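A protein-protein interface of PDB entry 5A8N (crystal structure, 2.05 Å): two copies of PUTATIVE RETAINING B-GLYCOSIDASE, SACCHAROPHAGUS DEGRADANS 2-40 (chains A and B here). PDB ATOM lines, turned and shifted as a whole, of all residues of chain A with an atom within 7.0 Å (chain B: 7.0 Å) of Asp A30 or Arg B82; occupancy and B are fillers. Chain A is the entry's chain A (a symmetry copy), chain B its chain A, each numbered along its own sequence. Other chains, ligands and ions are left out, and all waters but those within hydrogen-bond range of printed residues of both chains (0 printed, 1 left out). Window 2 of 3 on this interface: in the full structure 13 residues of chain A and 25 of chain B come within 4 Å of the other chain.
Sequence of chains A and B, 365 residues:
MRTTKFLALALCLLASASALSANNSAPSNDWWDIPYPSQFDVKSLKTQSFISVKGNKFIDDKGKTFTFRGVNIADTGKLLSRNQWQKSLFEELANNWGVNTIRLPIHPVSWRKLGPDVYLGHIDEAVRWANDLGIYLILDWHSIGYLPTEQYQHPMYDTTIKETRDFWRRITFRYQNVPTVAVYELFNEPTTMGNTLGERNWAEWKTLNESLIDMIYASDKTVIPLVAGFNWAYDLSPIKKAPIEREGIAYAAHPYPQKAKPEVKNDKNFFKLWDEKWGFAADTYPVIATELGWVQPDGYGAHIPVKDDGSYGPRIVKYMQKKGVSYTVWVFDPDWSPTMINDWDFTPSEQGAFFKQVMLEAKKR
Of the printed residues of chain B, Asn A29 touches Lys B113. Of the printed residues of chain B, Asp A30 touches Arg B82 (3.0 Å). Printed residues of chain A within 4 Å of Lys B78: Trp A32 (3.6 Å). Printed residues of chain A within 4 Å of Ser B81: Trp A32. Arg B82 touches two residues of chain A. Gln B86 touches none of the printed residues of chain A. Of the printed residues of chain A, Lys B113 touches Asn A29 (3.6 Å). Asp B335 touches none of the printed residues of chain A. The nearest residue of chain B that does not touch Asp A30 is Ser B81 (4.8 Å). The nearest residue of chain A that does not touch Arg B82 is Asp A33 (5.8 Å). The nearest printed residue of chain A that does not touch Ser B81 is Asp A30 (4.8 Å).
Of the 13 printed residues of chain B, 4 touch a printed residue of chain A. Printed residues of chain B that touch a printed residue of chain A: Lys B78, Ser B81, Arg B82 and Lys B113. Hydrophobic or aromatic side chains of chain A that line the printed part of chain B: Trp A32. Among the printed residues, Asp or Glu carboxylates within 4 Å of a Lys or Arg side-chain nitrogen of the other chain: Asp A30 with Arg B82 (3.0 Å).
The backbone carbonyl oxygen (O) of Lys B78 sits at hydrogen-bond distance from the side-chain hydroxyl (OG) of Ser B81. The side-chain carboxylate (OD2) of Asp B335 lies within salt-bridge range of the side-chain amino group (NZ) of Lys B78. The guanidinium group (NH1) of Arg B82 is in hydrogen-bond range of the side-chain hydroxyl (OG) of Ser B81 (2.7 Å).
The guanidinium group (NH2) of Arg B82 is in salt-bridge range of the side-chain carboxylate (OD2) of Asp A30, 3.0 Å away.
No position is printed for both chains.
Among the printed residues, pairs that only touch across the chains: Asn A29 with Lys B113 (3.6 Å), Trp A32 with Lys B78 (3.6 Å), Trp A32 with Ser B81 (3.8 Å) and Trp A32 with Arg B82 (3.7 Å).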
ATOM      1  N   ASN A  29     -14.951  -7.690 -28.300  1.00  0.00           N
ATOM      2  CA  ASN A  29     -15.546  -6.397 -28.775  1.00  0.00           C
ATOM      3  C   ASN A  29     -16.636  -5.878 -27.840  1.00  0.00           C
ATOM      4  O   ASN A  29     -17.838  -5.945 -28.152  1.00  0.00           O
ATOM      5  CB  ASN A  29     -16.125  -6.549 -30.184  1.00  0.00           C
ATOM      6  CG  ASN A  29     -15.055  -6.593 -31.261  1.00  0.00           C
ATOM      7  OD1 ASN A  29     -13.927  -6.127 -31.072  1.00  0.00           O
ATOM      8  ND2 ASN A  29     -15.417  -7.137 -32.414  1.00  0.00           N
ATOM      9  N   ASP A  30     -16.197  -5.389 -26.686  1.00  0.00           N
ATOM     10  CA  ASP A  30     -17.053  -4.737 -25.728  1.00  0.00           C
ATOM     11  C   ASP A  30     -16.833  -3.246 -25.905  1.00  0.00           C
ATOM     12  O   ASP A  30     -15.703  -2.750 -25.828  1.00  0.00           O
ATOM     13  CB  ASP A  30     -16.698  -5.143 -24.304  1.00  0.00           C
ATOM     14  CG  ASP A  30     -16.771  -6.643 -24.078  1.00  0.00           C
ATOM     15  OD1 ASP A  30     -17.788  -7.232 -24.440  1.00  0.00           O
ATOM     16  OD2 ASP A  30     -15.804  -7.232 -23.548  1.00  0.00           O
ATOM     17  N   TRP A  31     -17.921  -2.526 -26.126  1.00  0.00           N
ATOM     18  CA  TRP A  31     -17.838  -1.104 -26.470  1.00  0.00           C
ATOM     19  C   TRP A  31     -17.268  -0.258 -25.337  1.00  0.00           C
ATOM     20  O   TRP A  31     -16.662   0.784 -25.574  1.00  0.00           O
ATOM     21  CB  TRP A  31     -19.208  -0.594 -26.923  1.00  0.00           C
ATOM     22  CG  TRP A  31     -20.370  -1.012 -26.033  1.00  0.00           C
ATOM     23  CD1 TRP A  31     -21.261  -1.992 -26.285  1.00  0.00           C
ATOM     24  CD2 TRP A  31     -20.734  -0.451 -24.763  1.00  0.00           C
ATOM     25  NE1 TRP A  31     -22.172  -2.096 -25.259  1.00  0.00           N
ATOM     26  CE2 TRP A  31     -21.877  -1.149 -24.313  1.00  0.00           C
ATOM     27  CE3 TRP A  31     -20.223   0.590 -23.975  1.00  0.00           C
ATOM     28  CZ2 TRP A  31     -22.512  -0.849 -23.109  1.00  0.00           C
ATOM     29  CZ3 TRP A  31     -20.862   0.892 -22.766  1.00  0.00           C
ATOM     30  CH2 TRP A  31     -21.987   0.175 -22.352  1.00  0.00           C
ATOM     31  N   TRP A  32     -17.395  -0.750 -24.107  1.00  0.00           N
ATOM     32  CA  TRP A  32     -16.856  -0.023 -22.943  1.00  0.00           C
ATOM     33  C   TRP A  32     -15.330  -0.115 -22.844  1.00  0.00           C
ATOM     34  O   TRP A  32     -14.711   0.663 -22.123  1.00  0.00           O
ATOM     35  CB  TRP A  32     -17.531  -0.460 -21.633  1.00  0.00           C
ATOM     36  CG  TRP A  32     -17.399  -1.913 -21.334  1.00  0.00           C
ATOM     37  CD1 TRP A  32     -16.387  -2.519 -20.641  1.00  0.00           C
ATOM     38  CD2 TRP A  32     -18.304  -2.939 -21.708  1.00  0.00           C
ATOM     39  NE1 TRP A  32     -16.601  -3.865 -20.584  1.00  0.00           N
ATOM     40  CE2 TRP A  32     -17.778  -4.152 -21.223  1.00  0.00           C
ATOM     41  CE3 TRP A  32     -19.510  -2.959 -22.415  1.00  0.00           C
ATOM     42  CZ2 TRP A  32     -18.408  -5.369 -21.429  1.00  0.00           C
ATOM     43  CZ3 TRP A  32     -20.148  -4.181 -22.616  1.00  0.00           C
ATOM     44  CH2 TRP A  32     -19.590  -5.365 -22.137  1.00  0.00           C
ATOM     45  N   ASP A  33     -14.725  -1.029 -23.591  1.00  0.00           N
ATOM     46  CA  ASP A  33     -13.260  -1.157 -23.638  1.00  0.00           C
ATOM     47  C   ASP A  33     -12.602  -0.511 -24.866  1.00  0.00           C
ATOM     48  O   ASP A  33     -11.393  -0.604 -25.031  1.00  0.00           O
ATOM     49  CB  ASP A  33     -12.872  -2.648 -23.539  1.00  0.00           C
ATOM     50  CG  ASP A  33     -13.084  -3.208 -22.139  1.00  0.00           C
ATOM     51  OD1 ASP A  33     -13.101  -2.405 -21.172  1.00  0.00           O
ATOM     52  OD2 ASP A  33     -13.229  -4.438 -21.998  1.00  0.00           O
ATOM     53  N   ILE A  34     -13.385   0.140 -25.726  1.00  0.00           N
ATOM     54  CA  ILE A  34     -12.832   0.933 -26.835  1.00  0.00           C
ATOM     55  C   ILE A  34     -11.948   2.064 -26.276  1.00  0.00           C
ATOM     56  O   ILE A  34     -12.409   2.861 -25.466  1.00  0.00           O
ATOM     57  CB  ILE A  34     -13.955   1.552 -27.685  1.00  0.00           C
ATOM     58  CG1 ILE A  34     -14.693   0.447 -28.444  1.00  0.00           C
ATOM     59  CG2 ILE A  34     -13.404   2.604 -28.659  1.00  0.00           C
ATOM     60  CD1 ILE A  34     -15.906   0.939 -29.214  1.00  0.00           C
ATOM     61  N   GLY B  77     -26.889  -4.098 -21.576  1.00  0.00           N
ATOM     62  CA  GLY B  77     -26.117  -4.871 -22.550  1.00  0.00           C
ATOM     63  C   GLY B  77     -24.840  -5.440 -21.975  1.00  0.00           C
ATOM     64  O   GLY B  77     -24.480  -6.584 -22.252  1.00  0.00           O
ATOM     65  N   LYS B  78     -24.138  -4.675 -21.147  1.00  0.00           N
ATOM     66  CA  LYS B  78     -22.954  -5.231 -20.504  1.00  0.00           C
ATOM     67  C   LYS B  78     -23.339  -6.427 -19.603  1.00  0.00           C
ATOM     68  O   LYS B  78     -22.673  -7.482 -19.611  1.00  0.00           O
ATOM     69  CB  LYS B  78     -22.202  -4.168 -19.697  1.00  0.00           C
ATOM     70  CG  LYS B  78     -21.078  -4.757 -18.864  1.00  0.00           C
ATOM     71  CD  LYS B  78     -20.365  -3.735 -18.028  1.00  0.00           C
ATOM     72  CE  LYS B  78     -19.203  -4.376 -17.278  1.00  0.00           C
ATOM     73  NZ  LYS B  78     -19.631  -5.276 -16.187  1.00  0.00           N
ATOM     74  N   LEU B  79     -24.394  -6.260 -18.812  1.00  0.00           N
ATOM     75  CA  LEU B  79     -24.797  -7.316 -17.894  1.00  0.00           C
ATOM     76  C   LEU B  79     -25.241  -8.567 -18.653  1.00  0.00           C
ATOM     77  O   LEU B  79     -24.819  -9.678 -18.313  1.00  0.00           O
ATOM     78  CB  LEU B  79     -25.874  -6.827 -16.910  1.00  0.00           C
ATOM     79  CG  LEU B  79     -25.389  -5.726 -15.961  1.00  0.00           C
ATOM     80  CD1 LEU B  79     -26.511  -5.112 -15.140  1.00  0.00           C
ATOM     81  CD2 LEU B  79     -24.323  -6.285 -15.044  1.00  0.00           C
ATOM     82  N   LEU B  80     -26.051  -8.390 -19.690  1.00  0.00           N
ATOM     83  CA  LEU B  80     -26.511  -9.536 -20.493  1.00  0.00           C
ATOM     84  C   LEU B  80     -25.323 -10.309 -21.079  1.00  0.00           C
ATOM     85  O   LEU B  80     -25.316 -11.540 -21.084  1.00  0.00           O
ATOM     86  CB  LEU B  80     -27.411  -9.082 -21.639  1.00  0.00           C
ATOM     87  CG  LEU B  80     -28.849  -8.722 -21.309  1.00  0.00           C
ATOM     88  CD1 LEU B  80     -29.410  -7.863 -22.438  1.00  0.00           C
ATOM     89  CD2 LEU B  80     -29.652  -9.997 -21.134  1.00  0.00           C
ATOM     90  N   SER B  81     -24.304  -9.585 -21.528  1.00  0.00           N
ATOM     91  CA  SER B  81     -23.144 -10.208 -22.170  1.00  0.00           C
ATOM     92  C   SER B  81     -22.403 -11.167 -21.237  1.00  0.00           C
ATOM     93  O   SER B  81     -21.699 -12.045 -21.711  1.00  0.00           O
ATOM     94  CB  SER B  81     -22.168  -9.154 -22.698  1.00  0.00           C
ATOM     95  OG  SER B  81     -21.365  -8.676 -21.633  1.00  0.00           O
ATOM     96  N   ARG B  82     -22.553 -10.993 -19.918  1.00  0.00           N
ATOM     97  CA  ARG B  82     -21.925 -11.901 -18.969  1.00  0.00           C
ATOM     98  C   ARG B  82     -22.976 -12.691 -18.165  1.00  0.00           C
ATOM     99  O   ARG B  82     -22.664 -13.264 -17.130  1.00  0.00           O
ATOM    100  CB  ARG B  82     -20.961 -11.139 -18.032  1.00  0.00           C
ATOM    101  CG  ARG B  82     -19.834 -10.353 -18.719  1.00  0.00           C
ATOM    102  CD  ARG B  82     -19.102 -11.157 -19.786  1.00  0.00           C
ATOM    103  NE  ARG B  82     -17.816 -10.589 -20.233  1.00  0.00           N
ATOM    104  CZ  ARG B  82     -17.645  -9.656 -21.175  1.00  0.00           C
ATOM    105  NH1 ARG B  82     -18.672  -9.083 -21.796  1.00  0.00           N
ATOM    106  NH2 ARG B  82     -16.412  -9.266 -21.486  1.00  0.00           N
ATOM    107  N   ASN B  83     -24.212 -12.710 -18.653  1.00  0.00           N
ATOM    108  CA  ASN B  83     -25.312 -13.410 -17.990  1.00  0.00           C
ATOM    109  C   ASN B  83     -25.571 -12.942 -16.567  1.00  0.00           C
ATOM    110  O   ASN B  83     -25.934 -13.741 -15.703  1.00  0.00           O
ATOM    111  CB  ASN B  83     -25.069 -14.920 -17.974  1.00  0.00           C
ATOM    112  CG  ASN B  83     -24.932 -15.491 -19.362  1.00  0.00           C
ATOM    113  OD1 ASN B  83     -25.773 -15.254 -20.220  1.00  0.00           O
ATOM    114  ND2 ASN B  83     -23.871 -16.242 -19.597  1.00  0.00           N
ATOM    115  N   GLN B  84     -25.396 -11.647 -16.328  1.00  0.00           N
ATOM    116  CA  GLN B  84     -25.652 -11.070 -15.015  1.00  0.00           C
ATOM    117  C   GLN B  84     -26.899 -10.210 -14.987  1.00  0.00           C
ATOM    118  O   GLN B  84     -27.187  -9.604 -13.949  1.00  0.00           O
ATOM    119  CB  GLN B  84     -24.451 -10.240 -14.554  1.00  0.00           C
ATOM    120  CG  GLN B  84     -23.205 -11.079 -14.400  1.00  0.00           C
ATOM    121  CD  GLN B  84     -23.269 -12.030 -13.219  1.00  0.00           C
ATOM    122  OE1 GLN B  84     -24.084 -11.878 -12.301  1.00  0.00           O
ATOM    123  NE2 GLN B  84     -22.374 -12.992 -13.216  1.00  0.00           N
ATOM    124  N   TRP B  85     -27.631 -10.150 -16.111  1.00  0.00           N
ATOM    125  CA  TRP B  85     -28.923  -9.466 -16.156  1.00  0.00           C
ATOM    126  C   TRP B  85     -30.003 -10.441 -15.737  1.00  0.00           C
ATOM    127  O   TRP B  85     -30.494 -11.238 -16.538  1.00  0.00           O
ATOM    128  CB  TRP B  85     -29.230  -8.902 -17.537  1.00  0.00           C
ATOM    129  CG  TRP B  85     -30.483  -8.098 -17.595  1.00  0.00           C
ATOM    130  CD1 TRP B  85     -31.672  -8.503 -18.122  1.00  0.00           C
ATOM    131  CD2 TRP B  85     -30.704  -6.769 -17.100  1.00  0.00           C
ATOM    132  NE1 TRP B  85     -32.619  -7.506 -18.014  1.00  0.00           N
ATOM    133  CE2 TRP B  85     -32.051  -6.434 -17.386  1.00  0.00           C
ATOM    134  CE3 TRP B  85     -29.900  -5.819 -16.471  1.00  0.00           C
ATOM    135  CZ2 TRP B  85     -32.597  -5.203 -17.068  1.00  0.00           C
ATOM    136  CZ3 TRP B  85     -30.454  -4.587 -16.164  1.00  0.00           C
ATOM    137  CH2 TRP B  85     -31.785  -4.298 -16.453  1.00  0.00           C
ATOM    138  N   GLN B  86     -30.327 -10.370 -14.449  1.00  0.00           N
ATOM    139  CA  GLN B  86     -31.278 -11.281 -13.835  1.00  0.00           C
ATOM    140  C   GLN B  86     -31.838 -10.722 -12.523  1.00  0.00           C
ATOM    141  O   GLN B  86     -31.247  -9.845 -11.901  1.00  0.00           O
ATOM    142  CB  GLN B  86     -30.635 -12.647 -13.620  1.00  0.00           C
ATOM    143  CG  GLN B  86     -29.355 -12.622 -12.819  1.00  0.00           C
ATOM    144  CD  GLN B  86     -28.616 -13.938 -12.917  1.00  0.00           C
ATOM    145  OE1 GLN B  86     -29.065 -14.858 -13.598  1.00  0.00           O
ATOM    146  NE2 GLN B  86     -27.478 -14.031 -12.250  1.00  0.00           N
ATOM    147  N   LYS B 113     -26.928  -0.989 -30.378  1.00  0.00           N
ATOM    148  CA  LYS B 113     -26.466  -2.349 -30.570  1.00  0.00           C
ATOM    149  C   LYS B 113     -27.570  -3.382 -30.268  1.00  0.00           C
ATOM    150  O   LYS B 113     -27.825  -4.284 -31.062  1.00  0.00           O
ATOM    151  CB  LYS B 113     -25.268  -2.630 -29.677  1.00  0.00           C
ATOM    152  CG  LYS B 113     -24.637  -3.978 -29.946  1.00  0.00           C
ATOM    153  CD  LYS B 113     -23.312  -4.124 -29.235  1.00  0.00           C
ATOM    154  CE  LYS B 113     -22.565  -5.344 -29.766  1.00  0.00           C
ATOM    155  NZ  LYS B 113     -21.335  -5.509 -28.964  1.00  0.00           N
ATOM    156  N   ASP B 335     -16.429  -4.486 -12.662  1.00  0.00           N
ATOM    157  CA  ASP B 335     -15.511  -4.100 -13.760  1.00  0.00           C
ATOM    158  C   ASP B 335     -15.332  -2.591 -13.922  1.00  0.00           C
ATOM    159  O   ASP B 335     -14.220  -2.104 -14.081  1.00  0.00           O
ATOM    160  CB  ASP B 335     -16.017  -4.665 -15.078  1.00  0.00           C
ATOM    161  CG  ASP B 335     -16.229  -6.152 -15.011  1.00  0.00           C
ATOM    162  OD1 ASP B 335     -15.267  -6.812 -14.590  1.00  0.00           O
ATOM    163  OD2 ASP B 335     -17.331  -6.644 -15.376  1.00  0.00           O
ATOM    164  N   TRP B 344     -18.720 -10.941  -8.754  1.00  0.00           N
ATOM    165  CA  TRP B 344     -20.146 -11.215  -8.831  1.00  0.00           C
ATOM    166  C   TRP B 344     -20.697 -12.101  -7.721  1.00  0.00           C
ATOM    167  O   TRP B 344     -21.873 -12.450  -7.760  1.00  0.00           O
ATOM    168  CB  TRP B 344     -20.503 -11.790 -10.196  1.00  0.00           C
ATOM    169  CG  TRP B 344     -20.515 -10.732 -11.253  1.00  0.00           C
ATOM    170  CD1 TRP B 344     -19.726 -10.661 -12.355  1.00  0.00           C
ATOM    171  CD2 TRP B 344     -21.365  -9.581 -11.290  1.00  0.00           C
ATOM    172  NE1 TRP B 344     -20.035  -9.541 -13.089  1.00  0.00           N
ATOM    173  CE2 TRP B 344     -21.049  -8.866 -12.458  1.00  0.00           C
ATOM    174  CE3 TRP B 344     -22.377  -9.096 -10.452  1.00  0.00           C
ATOM    175  CZ2 TRP B 344     -21.692  -7.683 -12.804  1.00  0.00           C
ATOM    176  CZ3 TRP B 344     -23.032  -7.917 -10.809  1.00  0.00           C
ATOM    177  CH2 TRP B 344     -22.672  -7.221 -11.969  1.00  0.00           C
